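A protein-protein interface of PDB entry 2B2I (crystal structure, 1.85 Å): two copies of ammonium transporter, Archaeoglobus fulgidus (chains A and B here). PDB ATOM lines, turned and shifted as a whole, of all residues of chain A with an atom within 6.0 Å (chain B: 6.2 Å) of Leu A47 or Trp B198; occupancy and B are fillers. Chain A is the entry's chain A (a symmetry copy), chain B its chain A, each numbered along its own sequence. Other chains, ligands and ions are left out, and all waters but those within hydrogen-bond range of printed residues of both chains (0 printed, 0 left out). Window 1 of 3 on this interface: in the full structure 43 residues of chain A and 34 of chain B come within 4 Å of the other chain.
The indole nitrogen (NE1) of Trp B198 sits at hydrogen-bond distance from the side-chain amide oxygen (OD1) of Asn B224 (3.0 Å).
Among the printed residues, merely in contact across the chains: Ile A48 with Ala B228 (3.2 Å), Pro A21 with Ala B195 (3.5 Å), Met A95 with Asn B224 (3.5 Å), Met A17 with Phe B202 (3.6 Å), Leu A47 with Trp B198 (3.6 Å), Val A51 with Ala B228 (3.7 Å), Met A17 with Phe B199 (3.7 Å), Met A17 with Trp B198 (3.8 Å), Leu A52 with Ala B228 (3.8 Å), Val A51 with Asn B224 (3.8 Å) and Phe A44 with Ala B195 (3.96 Å).
Printed residues of chain B within 4 Å of Phe A44: Ala B195 (3.96 Å).
Leu A47 touches just one residue of chain B: Trp B198 (3.6 Å).
Of the printed residues of chain A, Ala B195 touches Pro A21 and Phe A44.
Trp B198 touches just these residues of chain A: Met A17 and Leu A47.
The nearest residue of chain A that does not touch Trp B198 is Ile A48 (4.3 Å).
Of the 16 printed residues of chain A, 8 touch a printed residue of chain B.
Hydrophobic or aromatic side chains of chain B that line the printed part of chain A: Ala B195, Trp B198, Phe B199, Phe B202 and Ala B228.
Among the printed residues, 11 pairs touch across the chains.
Among the printed residues, no Asp or Glu carboxylate lies within 4 Å of a Lys or Arg side-chain nitrogen of the other chain.
No position is printed for both chains.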
ATOM      1  N   MET A  17     -15.129 -25.379  13.605  1.00  0.00           N
ATOM      2  CA  MET A  17     -15.327 -25.072  15.019  1.00  0.00           C
ATOM      3  C   MET A  17     -14.934 -26.287  15.835  1.00  0.00           C
ATOM      4  O   MET A  17     -14.263 -26.179  16.861  1.00  0.00           O
ATOM      5  CB  MET A  17     -16.794 -24.722  15.284  1.00  0.00           C
ATOM      6  CG  MET A  17     -17.181 -24.604  16.747  1.00  0.00           C
ATOM      7  SD  MET A  17     -17.661 -26.185  17.454  1.00  0.00           S
ATOM      8  CE  MET A  17     -16.786 -26.105  19.058  1.00  0.00           C
ATOM      9  N   VAL A  20     -11.374 -26.890  17.015  1.00  0.00           N
ATOM     10  CA  VAL A  20     -10.777 -26.167  18.142  1.00  0.00           C
ATOM     11  C   VAL A  20     -10.650 -27.094  19.347  1.00  0.00           C
ATOM     12  O   VAL A  20      -9.542 -27.302  19.848  1.00  0.00           O
ATOM     13  CB  VAL A  20     -11.578 -24.909  18.511  1.00  0.00           C
ATOM     14  CG1 VAL A  20     -10.940 -24.212  19.715  1.00  0.00           C
ATOM     15  CG2 VAL A  20     -11.628 -23.970  17.323  1.00  0.00           C
ATOM     16  N   PRO A  21     -11.772 -27.650  19.846  1.00  0.00           N
ATOM     17  CA  PRO A  21     -11.570 -28.549  20.995  1.00  0.00           C
ATOM     18  C   PRO A  21     -10.824 -29.788  20.503  1.00  0.00           C
ATOM     19  O   PRO A  21     -10.105 -30.439  21.258  1.00  0.00           O
ATOM     20  CB  PRO A  21     -12.992 -28.859  21.462  1.00  0.00           C
ATOM     21  CG  PRO A  21     -13.829 -28.663  20.201  1.00  0.00           C
ATOM     22  CD  PRO A  21     -13.205 -27.423  19.588  1.00  0.00           C
ATOM     23  N   LEU A  42      -7.653 -24.773  27.557  1.00  0.00           N
ATOM     24  CA  LEU A  42      -7.013 -23.761  26.727  1.00  0.00           C
ATOM     25  C   LEU A  42      -7.638 -23.648  25.349  1.00  0.00           C
ATOM     26  O   LEU A  42      -7.761 -22.547  24.812  1.00  0.00           O
ATOM     27  CB  LEU A  42      -5.512 -24.048  26.594  1.00  0.00           C
ATOM     28  CG  LEU A  42      -4.671 -23.725  27.839  1.00  0.00           C
ATOM     29  CD1 LEU A  42      -3.194 -24.073  27.616  1.00  0.00           C
ATOM     30  CD2 LEU A  42      -4.810 -22.237  28.161  1.00  0.00           C
ATOM     31  N   SER A  43      -8.031 -24.781  24.770  1.00  0.00           N
ATOM     32  CA  SER A  43      -8.633 -24.756  23.440  1.00  0.00           C
ATOM     33  C   SER A  43     -10.019 -24.121  23.506  1.00  0.00           C
ATOM     34  O   SER A  43     -10.421 -23.409  22.591  1.00  0.00           O
ATOM     35  CB  SER A  43      -8.707 -26.166  22.837  1.00  0.00           C
ATOM     36  OG  SER A  43      -9.677 -26.976  23.496  1.00  0.00           O
ATOM     37  N   PHE A  44     -10.754 -24.362  24.587  1.00  0.00           N
ATOM     38  CA  PHE A  44     -12.078 -23.754  24.705  1.00  0.00           C
ATOM     39  C   PHE A  44     -11.939 -22.239  24.918  1.00  0.00           C
ATOM     40  O   PHE A  44     -12.670 -21.441  24.325  1.00  0.00           O
ATOM     41  CB  PHE A  44     -12.876 -24.375  25.858  1.00  0.00           C
ATOM     42  CG  PHE A  44     -13.562 -25.666  25.502  1.00  0.00           C
ATOM     43  CD1 PHE A  44     -12.947 -26.891  25.740  1.00  0.00           C
ATOM     44  CD2 PHE A  44     -14.820 -25.652  24.906  1.00  0.00           C
ATOM     45  CE1 PHE A  44     -13.573 -28.087  25.391  1.00  0.00           C
ATOM     46  CE2 PHE A  44     -15.456 -26.840  24.553  1.00  0.00           C
ATOM     47  CZ  PHE A  44     -14.828 -28.067  24.798  1.00  0.00           C
ATOM     48  N   ILE A  45     -11.001 -21.844  25.773  1.00  0.00           N
ATOM     49  CA  ILE A  45     -10.756 -20.431  26.029  1.00  0.00           C
ATOM     50  C   ILE A  45     -10.376 -19.757  24.710  1.00  0.00           C
ATOM     51  O   ILE A  45     -10.867 -18.675  24.392  1.00  0.00           O
ATOM     52  CB  ILE A  45      -9.626 -20.276  27.065  1.00  0.00           C
ATOM     53  CG1 ILE A  45     -10.082 -20.905  28.386  1.00  0.00           C
ATOM     54  CG2 ILE A  45      -9.251 -18.813  27.234  1.00  0.00           C
ATOM     55  CD1 ILE A  45      -9.012 -20.907  29.474  1.00  0.00           C
ATOM     56  N   SER A  46      -9.511 -20.413  23.939  1.00  0.00           N
ATOM     57  CA  SER A  46      -9.085 -19.888  22.640  1.00  0.00           C
ATOM     58  C   SER A  46     -10.309 -19.577  21.792  1.00  0.00           C
ATOM     59  O   SER A  46     -10.394 -18.537  21.144  1.00  0.00           O
ATOM     60  CB  SER A  46      -8.225 -20.920  21.906  1.00  0.00           C
ATOM     61  OG  SER A  46      -7.037 -21.198  22.623  1.00  0.00           O
ATOM     62  N   LEU A  47     -11.258 -20.498  21.795  1.00  0.00           N
ATOM     63  CA  LEU A  47     -12.471 -20.316  21.026  1.00  0.00           C
ATOM     64  C   LEU A  47     -13.241 -19.092  21.544  1.00  0.00           C
ATOM     65  O   LEU A  47     -13.511 -18.150  20.792  1.00  0.00           O
ATOM     66  CB  LEU A  47     -13.346 -21.567  21.131  1.00  0.00           C
ATOM     67  CG  LEU A  47     -14.647 -21.486  20.326  1.00  0.00           C
ATOM     68  CD1 LEU A  47     -14.304 -21.267  18.868  1.00  0.00           C
ATOM     69  CD2 LEU A  47     -15.460 -22.768  20.490  1.00  0.00           C
ATOM     70  N   ILE A  48     -13.570 -19.110  22.835  1.00  0.00           N
ATOM     71  CA  ILE A  48     -14.316 -18.023  23.464  1.00  0.00           C
ATOM     72  C   ILE A  48     -13.678 -16.671  23.220  1.00  0.00           C
ATOM     73  O   ILE A  48     -14.333 -15.735  22.763  1.00  0.00           O
ATOM     74  CB  ILE A  48     -14.436 -18.250  24.967  1.00  0.00           C
ATOM     75  CG1 ILE A  48     -15.227 -19.541  25.203  1.00  0.00           C
ATOM     76  CG2 ILE A  48     -15.119 -17.043  25.633  1.00  0.00           C
ATOM     77  CD1 ILE A  48     -15.233 -20.008  26.636  1.00  0.00           C
ATOM     78  N   ILE A  49     -12.394 -16.573  23.521  1.00  0.00           N
ATOM     79  CA  ILE A  49     -11.671 -15.328  23.332  1.00  0.00           C
ATOM     80  C   ILE A  49     -11.707 -14.907  21.860  1.00  0.00           C
ATOM     81  O   ILE A  49     -12.027 -13.758  21.542  1.00  0.00           O
ATOM     82  CB  ILE A  49     -10.204 -15.491  23.820  1.00  0.00           C
ATOM     83  CG1 ILE A  49     -10.100 -15.106  25.296  1.00  0.00           C
ATOM     84  CG2 ILE A  49      -9.259 -14.626  23.005  1.00  0.00           C
ATOM     85  CD1 ILE A  49     -11.210 -15.648  26.173  1.00  0.00           C
ATOM     86  N   THR A  50     -11.397 -15.837  20.963  1.00  0.00           N
ATOM     87  CA  THR A  50     -11.388 -15.535  19.539  1.00  0.00           C
ATOM     88  C   THR A  50     -12.711 -14.979  19.032  1.00  0.00           C
ATOM     89  O   THR A  50     -12.749 -13.964  18.330  1.00  0.00           O
ATOM     90  CB  THR A  50     -11.016 -16.775  18.733  1.00  0.00           C
ATOM     91  OG1 THR A  50      -9.670 -17.145  19.054  1.00  0.00           O
ATOM     92  CG2 THR A  50     -11.121 -16.501  17.244  1.00  0.00           C
ATOM     93  N   VAL A  51     -13.802 -15.646  19.381  1.00  0.00           N
ATOM     94  CA  VAL A  51     -15.117 -15.197  18.949  1.00  0.00           C
ATOM     95  C   VAL A  51     -15.381 -13.748  19.366  1.00  0.00           C
ATOM     96  O   VAL A  51     -15.857 -12.941  18.565  1.00  0.00           O
ATOM     97  CB  VAL A  51     -16.237 -16.071  19.544  1.00  0.00           C
ATOM     98  CG1 VAL A  51     -17.593 -15.483  19.172  1.00  0.00           C
ATOM     99  CG2 VAL A  51     -16.110 -17.504  19.038  1.00  0.00           C
ATOM    100  N   LEU A  52     -15.069 -13.418  20.615  1.00  0.00           N
ATOM    101  CA  LEU A  52     -15.302 -12.066  21.112  1.00  0.00           C
ATOM    102  C   LEU A  52     -14.453 -11.023  20.374  1.00  0.00           C
ATOM    103  O   LEU A  52     -14.985 -10.056  19.835  1.00  0.00           O
ATOM    104  CB  LEU A  52     -15.037 -12.012  22.624  1.00  0.00           C
ATOM    105  CG  LEU A  52     -15.879 -13.005  23.444  1.00  0.00           C
ATOM    106  CD1 LEU A  52     -15.455 -13.006  24.913  1.00  0.00           C
ATOM    107  CD2 LEU A  52     -17.339 -12.647  23.308  1.00  0.00           C
ATOM    108  N   MET A  95     -13.582 -18.999  12.749  1.00  0.00           N
ATOM    109  CA  MET A  95     -13.167 -20.323  13.204  1.00  0.00           C
ATOM    110  C   MET A  95     -11.718 -20.652  12.840  1.00  0.00           C
ATOM    111  O   MET A  95     -11.055 -21.410  13.553  1.00  0.00           O
ATOM    112  CB  MET A  95     -14.135 -21.391  12.677  1.00  0.00           C
ATOM    113  CG  MET A  95     -15.560 -21.212  13.214  1.00  0.00           C
ATOM    114  SD  MET A  95     -15.617 -21.167  15.056  1.00  0.00           S
ATOM    115  CE  MET A  95     -17.250 -20.502  15.326  1.00  0.00           C
ATOM    116  N   ALA A  98      -9.608 -19.169  15.554  1.00  0.00           N
ATOM    117  CA  ALA A  98      -9.711 -19.957  16.782  1.00  0.00           C
ATOM    118  C   ALA A  98      -8.824 -21.202  16.758  1.00  0.00           C
ATOM    119  O   ALA A  98      -8.169 -21.538  17.750  1.00  0.00           O
ATOM    120  CB  ALA A  98     -11.167 -20.366  17.009  1.00  0.00           C
ATOM    121  N   MET B  19     -25.987 -34.633  19.334  1.00  0.00           N
ATOM    122  CA  MET B  19     -26.120 -33.963  20.611  1.00  0.00           C
ATOM    123  C   MET B  19     -26.723 -34.877  21.679  1.00  0.00           C
ATOM    124  O   MET B  19     -26.527 -34.639  22.868  1.00  0.00           O
ATOM    125  CB  MET B  19     -26.970 -32.693  20.454  1.00  0.00           C
ATOM    126  CG  MET B  19     -26.318 -31.625  19.596  1.00  0.00           C
ATOM    127  SD  MET B  19     -27.362 -30.164  19.401  1.00  0.00           S
ATOM    128  CE  MET B  19     -27.192 -29.421  20.945  1.00  0.00           C
ATOM    129  N   GLY B 193     -18.060 -34.202  25.656  1.00  0.00           N
ATOM    130  CA  GLY B 193     -19.489 -34.014  25.517  1.00  0.00           C
ATOM    131  C   GLY B 193     -19.761 -32.566  25.141  1.00  0.00           C
ATOM    132  O   GLY B 193     -20.522 -32.285  24.212  1.00  0.00           O
ATOM    133  N   ALA B 194     -19.121 -31.640  25.853  1.00  0.00           N
ATOM    134  CA  ALA B 194     -19.302 -30.211  25.606  1.00  0.00           C
ATOM    135  C   ALA B 194     -18.929 -29.787  24.185  1.00  0.00           C
ATOM    136  O   ALA B 194     -19.611 -28.953  23.585  1.00  0.00           O
ATOM    137  CB  ALA B 194     -18.488 -29.409  26.614  1.00  0.00           C
ATOM    138  N   ALA B 195     -17.850 -30.349  23.644  1.00  0.00           N
ATOM    139  CA  ALA B 195     -17.447 -30.014  22.281  1.00  0.00           C
ATOM    140  C   ALA B 195     -18.489 -30.531  21.298  1.00  0.00           C
ATOM    141  O   ALA B 195     -18.792 -29.859  20.319  1.00  0.00           O
ATOM    142  CB  ALA B 195     -16.080 -30.605  21.966  1.00  0.00           C
ATOM    143  N   LEU B 196     -19.052 -31.708  21.565  1.00  0.00           N
ATOM    144  CA  LEU B 196     -20.078 -32.283  20.681  1.00  0.00           C
ATOM    145  C   LEU B 196     -21.389 -31.493  20.726  1.00  0.00           C
ATOM    146  O   LEU B 196     -22.128 -31.437  19.745  1.00  0.00           O
ATOM    147  CB  LEU B 196     -20.372 -33.739  21.061  1.00  0.00           C
ATOM    148  CG  LEU B 196     -19.210 -34.739  20.999  1.00  0.00           C
ATOM    149  CD1 LEU B 196     -19.748 -36.150  21.171  1.00  0.00           C
ATOM    150  CD2 LEU B 196     -18.489 -34.607  19.663  1.00  0.00           C
ATOM    151  N   LEU B 197     -21.678 -30.903  21.878  1.00  0.00           N
ATOM    152  CA  LEU B 197     -22.879 -30.108  22.043  1.00  0.00           C
ATOM    153  C   LEU B 197     -22.723 -28.767  21.348  1.00  0.00           C
ATOM    154  O   LEU B 197     -23.655 -28.288  20.700  1.00  0.00           O
ATOM    155  CB  LEU B 197     -23.173 -29.903  23.532  1.00  0.00           C
ATOM    156  CG  LEU B 197     -23.596 -31.208  24.227  1.00  0.00           C
ATOM    157  CD1 LEU B 197     -23.613 -31.006  25.732  1.00  0.00           C
ATOM    158  CD2 LEU B 197     -24.973 -31.641  23.716  1.00  0.00           C
ATOM    159  N   TRP B 198     -21.555 -28.143  21.474  1.00  0.00           N
ATOM    160  CA  TRP B 198     -21.351 -26.853  20.815  1.00  0.00           C
ATOM    161  C   TRP B 198     -21.426 -27.073  19.309  1.00  0.00           C
ATOM    162  O   TRP B 198     -22.145 -26.368  18.589  1.00  0.00           O
ATOM    163  CB  TRP B 198     -19.991 -26.263  21.172  1.00  0.00           C
ATOM    164  CG  TRP B 198     -19.855 -24.797  20.809  1.00  0.00           C
ATOM    165  CD1 TRP B 198     -20.263 -24.192  19.652  1.00  0.00           C
ATOM    166  CD2 TRP B 198     -19.217 -23.777  21.589  1.00  0.00           C
ATOM    167  NE1 TRP B 198     -19.914 -22.862  19.662  1.00  0.00           N
ATOM    168  CE2 TRP B 198     -19.269 -22.579  20.837  1.00  0.00           C
ATOM    169  CE3 TRP B 198     -18.602 -23.758  22.849  1.00  0.00           C
ATOM    170  CZ2 TRP B 198     -18.726 -21.372  21.304  1.00  0.00           C
ATOM    171  CZ3 TRP B 198     -18.062 -22.552  23.316  1.00  0.00           C
ATOM    172  CH2 TRP B 198     -18.128 -21.380  22.540  1.00  0.00           C
ATOM    173  N   PHE B 199     -20.682 -28.061  18.833  1.00  0.00           N
ATOM    174  CA  PHE B 199     -20.669 -28.393  17.419  1.00  0.00           C
ATOM    175  C   PHE B 199     -22.089 -28.720  16.927  1.00  0.00           C
ATOM    176  O   PHE B 199     -22.547 -28.177  15.926  1.00  0.00           O
ATOM    177  CB  PHE B 199     -19.719 -29.575  17.226  1.00  0.00           C
ATOM    178  CG  PHE B 199     -19.771 -30.209  15.864  1.00  0.00           C
ATOM    179  CD1 PHE B 199     -19.388 -29.503  14.725  1.00  0.00           C
ATOM    180  CD2 PHE B 199     -20.178 -31.539  15.731  1.00  0.00           C
ATOM    181  CE1 PHE B 199     -19.403 -30.114  13.469  1.00  0.00           C
ATOM    182  CE2 PHE B 199     -20.199 -32.161  14.495  1.00  0.00           C
ATOM    183  CZ  PHE B 199     -19.809 -31.445  13.351  1.00  0.00           C
ATOM    184  N   GLY B 200     -22.797 -29.588  17.642  1.00  0.00           N
ATOM    185  CA  GLY B 200     -24.145 -29.966  17.234  1.00  0.00           C
ATOM    186  C   GLY B 200     -25.146 -28.819  17.211  1.00  0.00           C
ATOM    187  O   GLY B 200     -26.108 -28.828  16.434  1.00  0.00           O
ATOM    188  N   TRP B 201     -24.919 -27.822  18.060  1.00  0.00           N
ATOM    189  CA  TRP B 201     -25.818 -26.684  18.139  1.00  0.00           C
ATOM    190  C   TRP B 201     -25.847 -25.866  16.845  1.00  0.00           C
ATOM    191  O   TRP B 201     -26.699 -25.002  16.685  1.00  0.00           O
ATOM    192  CB  TRP B 201     -25.432 -25.794  19.314  1.00  0.00           C
ATOM    193  CG  TRP B 201     -26.619 -25.346  20.113  1.00  0.00           C
ATOM    194  CD1 TRP B 201     -27.680 -24.580  19.681  1.00  0.00           C
ATOM    195  CD2 TRP B 201     -26.867 -25.637  21.492  1.00  0.00           C
ATOM    196  NE1 TRP B 201     -28.571 -24.381  20.717  1.00  0.00           N
ATOM    197  CE2 TRP B 201     -28.097 -25.016  21.831  1.00  0.00           C
ATOM    198  CE3 TRP B 201     -26.170 -26.360  22.466  1.00  0.00           C
ATOM    199  CZ2 TRP B 201     -28.637 -25.106  23.118  1.00  0.00           C
ATOM    200  CZ3 TRP B 201     -26.710 -26.449  23.741  1.00  0.00           C
ATOM    201  CH2 TRP B 201     -27.937 -25.822  24.056  1.00  0.00           C
ATOM    202  N   PHE B 202     -24.908 -26.139  15.937  1.00  0.00           N
ATOM    203  CA  PHE B 202     -24.864 -25.460  14.642  1.00  0.00           C
ATOM    204  C   PHE B 202     -26.087 -25.940  13.863  1.00  0.00           C
ATOM    205  O   PHE B 202     -26.748 -25.159  13.174  1.00  0.00           O
ATOM    206  CB  PHE B 202     -23.598 -25.840  13.873  1.00  0.00           C
ATOM    207  CG  PHE B 202     -22.407 -24.965  14.173  1.00  0.00           C
ATOM    208  CD1 PHE B 202     -22.047 -23.938  13.310  1.00  0.00           C
ATOM    209  CD2 PHE B 202     -21.645 -25.168  15.314  1.00  0.00           C
ATOM    210  CE1 PHE B 202     -20.935 -23.123  13.580  1.00  0.00           C
ATOM    211  CE2 PHE B 202     -20.538 -24.364  15.590  1.00  0.00           C
ATOM    212  CZ  PHE B 202     -20.186 -23.334  14.718  1.00  0.00           C
ATOM    213  N   THR B 223     -25.632 -17.468  17.725  1.00  0.00           N
ATOM    214  CA  THR B 223     -25.504 -18.615  18.609  1.00  0.00           C
ATOM    215  C   THR B 223     -24.089 -18.677  19.165  1.00  0.00           C
ATOM    216  O   THR B 223     -23.891 -18.827  20.370  1.00  0.00           O
ATOM    217  CB  THR B 223     -25.820 -19.926  17.871  1.00  0.00           C
ATOM    218  OG1 THR B 223     -27.210 -19.952  17.530  1.00  0.00           O
ATOM    219  CG2 THR B 223     -25.483 -21.132  18.751  1.00  0.00           C
ATOM    220  N   ASN B 224     -23.104 -18.559  18.280  1.00  0.00           N
ATOM    221  CA  ASN B 224     -21.715 -18.585  18.698  1.00  0.00           C
ATOM    222  C   ASN B 224     -21.395 -17.387  19.580  1.00  0.00           C
ATOM    223  O   ASN B 224     -20.584 -17.478  20.495  1.00  0.00           O
ATOM    224  CB  ASN B 224     -20.803 -18.605  17.477  1.00  0.00           C
ATOM    225  CG  ASN B 224     -20.686 -19.994  16.869  1.00  0.00           C
ATOM    226  OD1 ASN B 224     -20.059 -20.878  17.453  1.00  0.00           O
ATOM    227  ND2 ASN B 224     -21.300 -20.199  15.702  1.00  0.00           N
ATOM    228  N   ALA B 227     -22.886 -17.846  23.236  1.00  0.00           N
ATOM    229  CA  ALA B 227     -22.127 -18.894  23.908  1.00  0.00           C
ATOM    230  C   ALA B 227     -20.813 -18.332  24.445  1.00  0.00           C
ATOM    231  O   ALA B 227     -20.446 -18.570  25.602  1.00  0.00           O
ATOM    232  CB  ALA B 227     -21.855 -20.049  22.939  1.00  0.00           C
ATOM    233  N   ALA B 228     -20.119 -17.572  23.600  1.00  0.00           N
ATOM    234  CA  ALA B 228     -18.831 -16.985  23.962  1.00  0.00           C
ATOM    235  C   ALA B 228     -18.954 -16.001  25.112  1.00  0.00           C
ATOM    236  O   ALA B 228     -18.125 -15.986  26.028  1.00  0.00           O
ATOM    237  CB  ALA B 228     -18.218 -16.300  22.749  1.00  0.00           C
ATOM    238  N   ALA B 253     -20.924 -21.442  28.691  1.00  0.00           N
ATOM    239  CA  ALA B 253     -21.142 -21.437  27.252  1.00  0.00           C
ATOM    240  C   ALA B 253     -22.499 -22.056  26.925  1.00  0.00           C
ATOM    241  O   ALA B 253     -23.215 -21.574  26.048  1.00  0.00           O
ATOM    242  CB  ALA B 253     -20.016 -22.201  26.529  1.00  0.00           C
ATOM    243  N   LEU B 257     -25.864 -20.720  25.000  1.00  0.00           N
ATOM    244  CA  LEU B 257     -26.449 -21.439  23.869  1.00  0.00           C
ATOM    245  C   LEU B 257     -27.952 -21.664  24.079  1.00  0.00           C
ATOM    246  O   LEU B 257     -28.754 -21.493  23.155  1.00  0.00           O
ATOM    247  CB  LEU B 257     -25.725 -22.781  23.656  1.00  0.00           C
ATOM    248  CG  LEU B 257     -24.277 -22.684  23.144  1.00  0.00           C
ATOM    249  CD1 LEU B 257     -23.583 -24.040  23.252  1.00  0.00           C
ATOM    250  CD2 LEU B 257     -24.288 -22.200  21.693  1.00  0.00           C
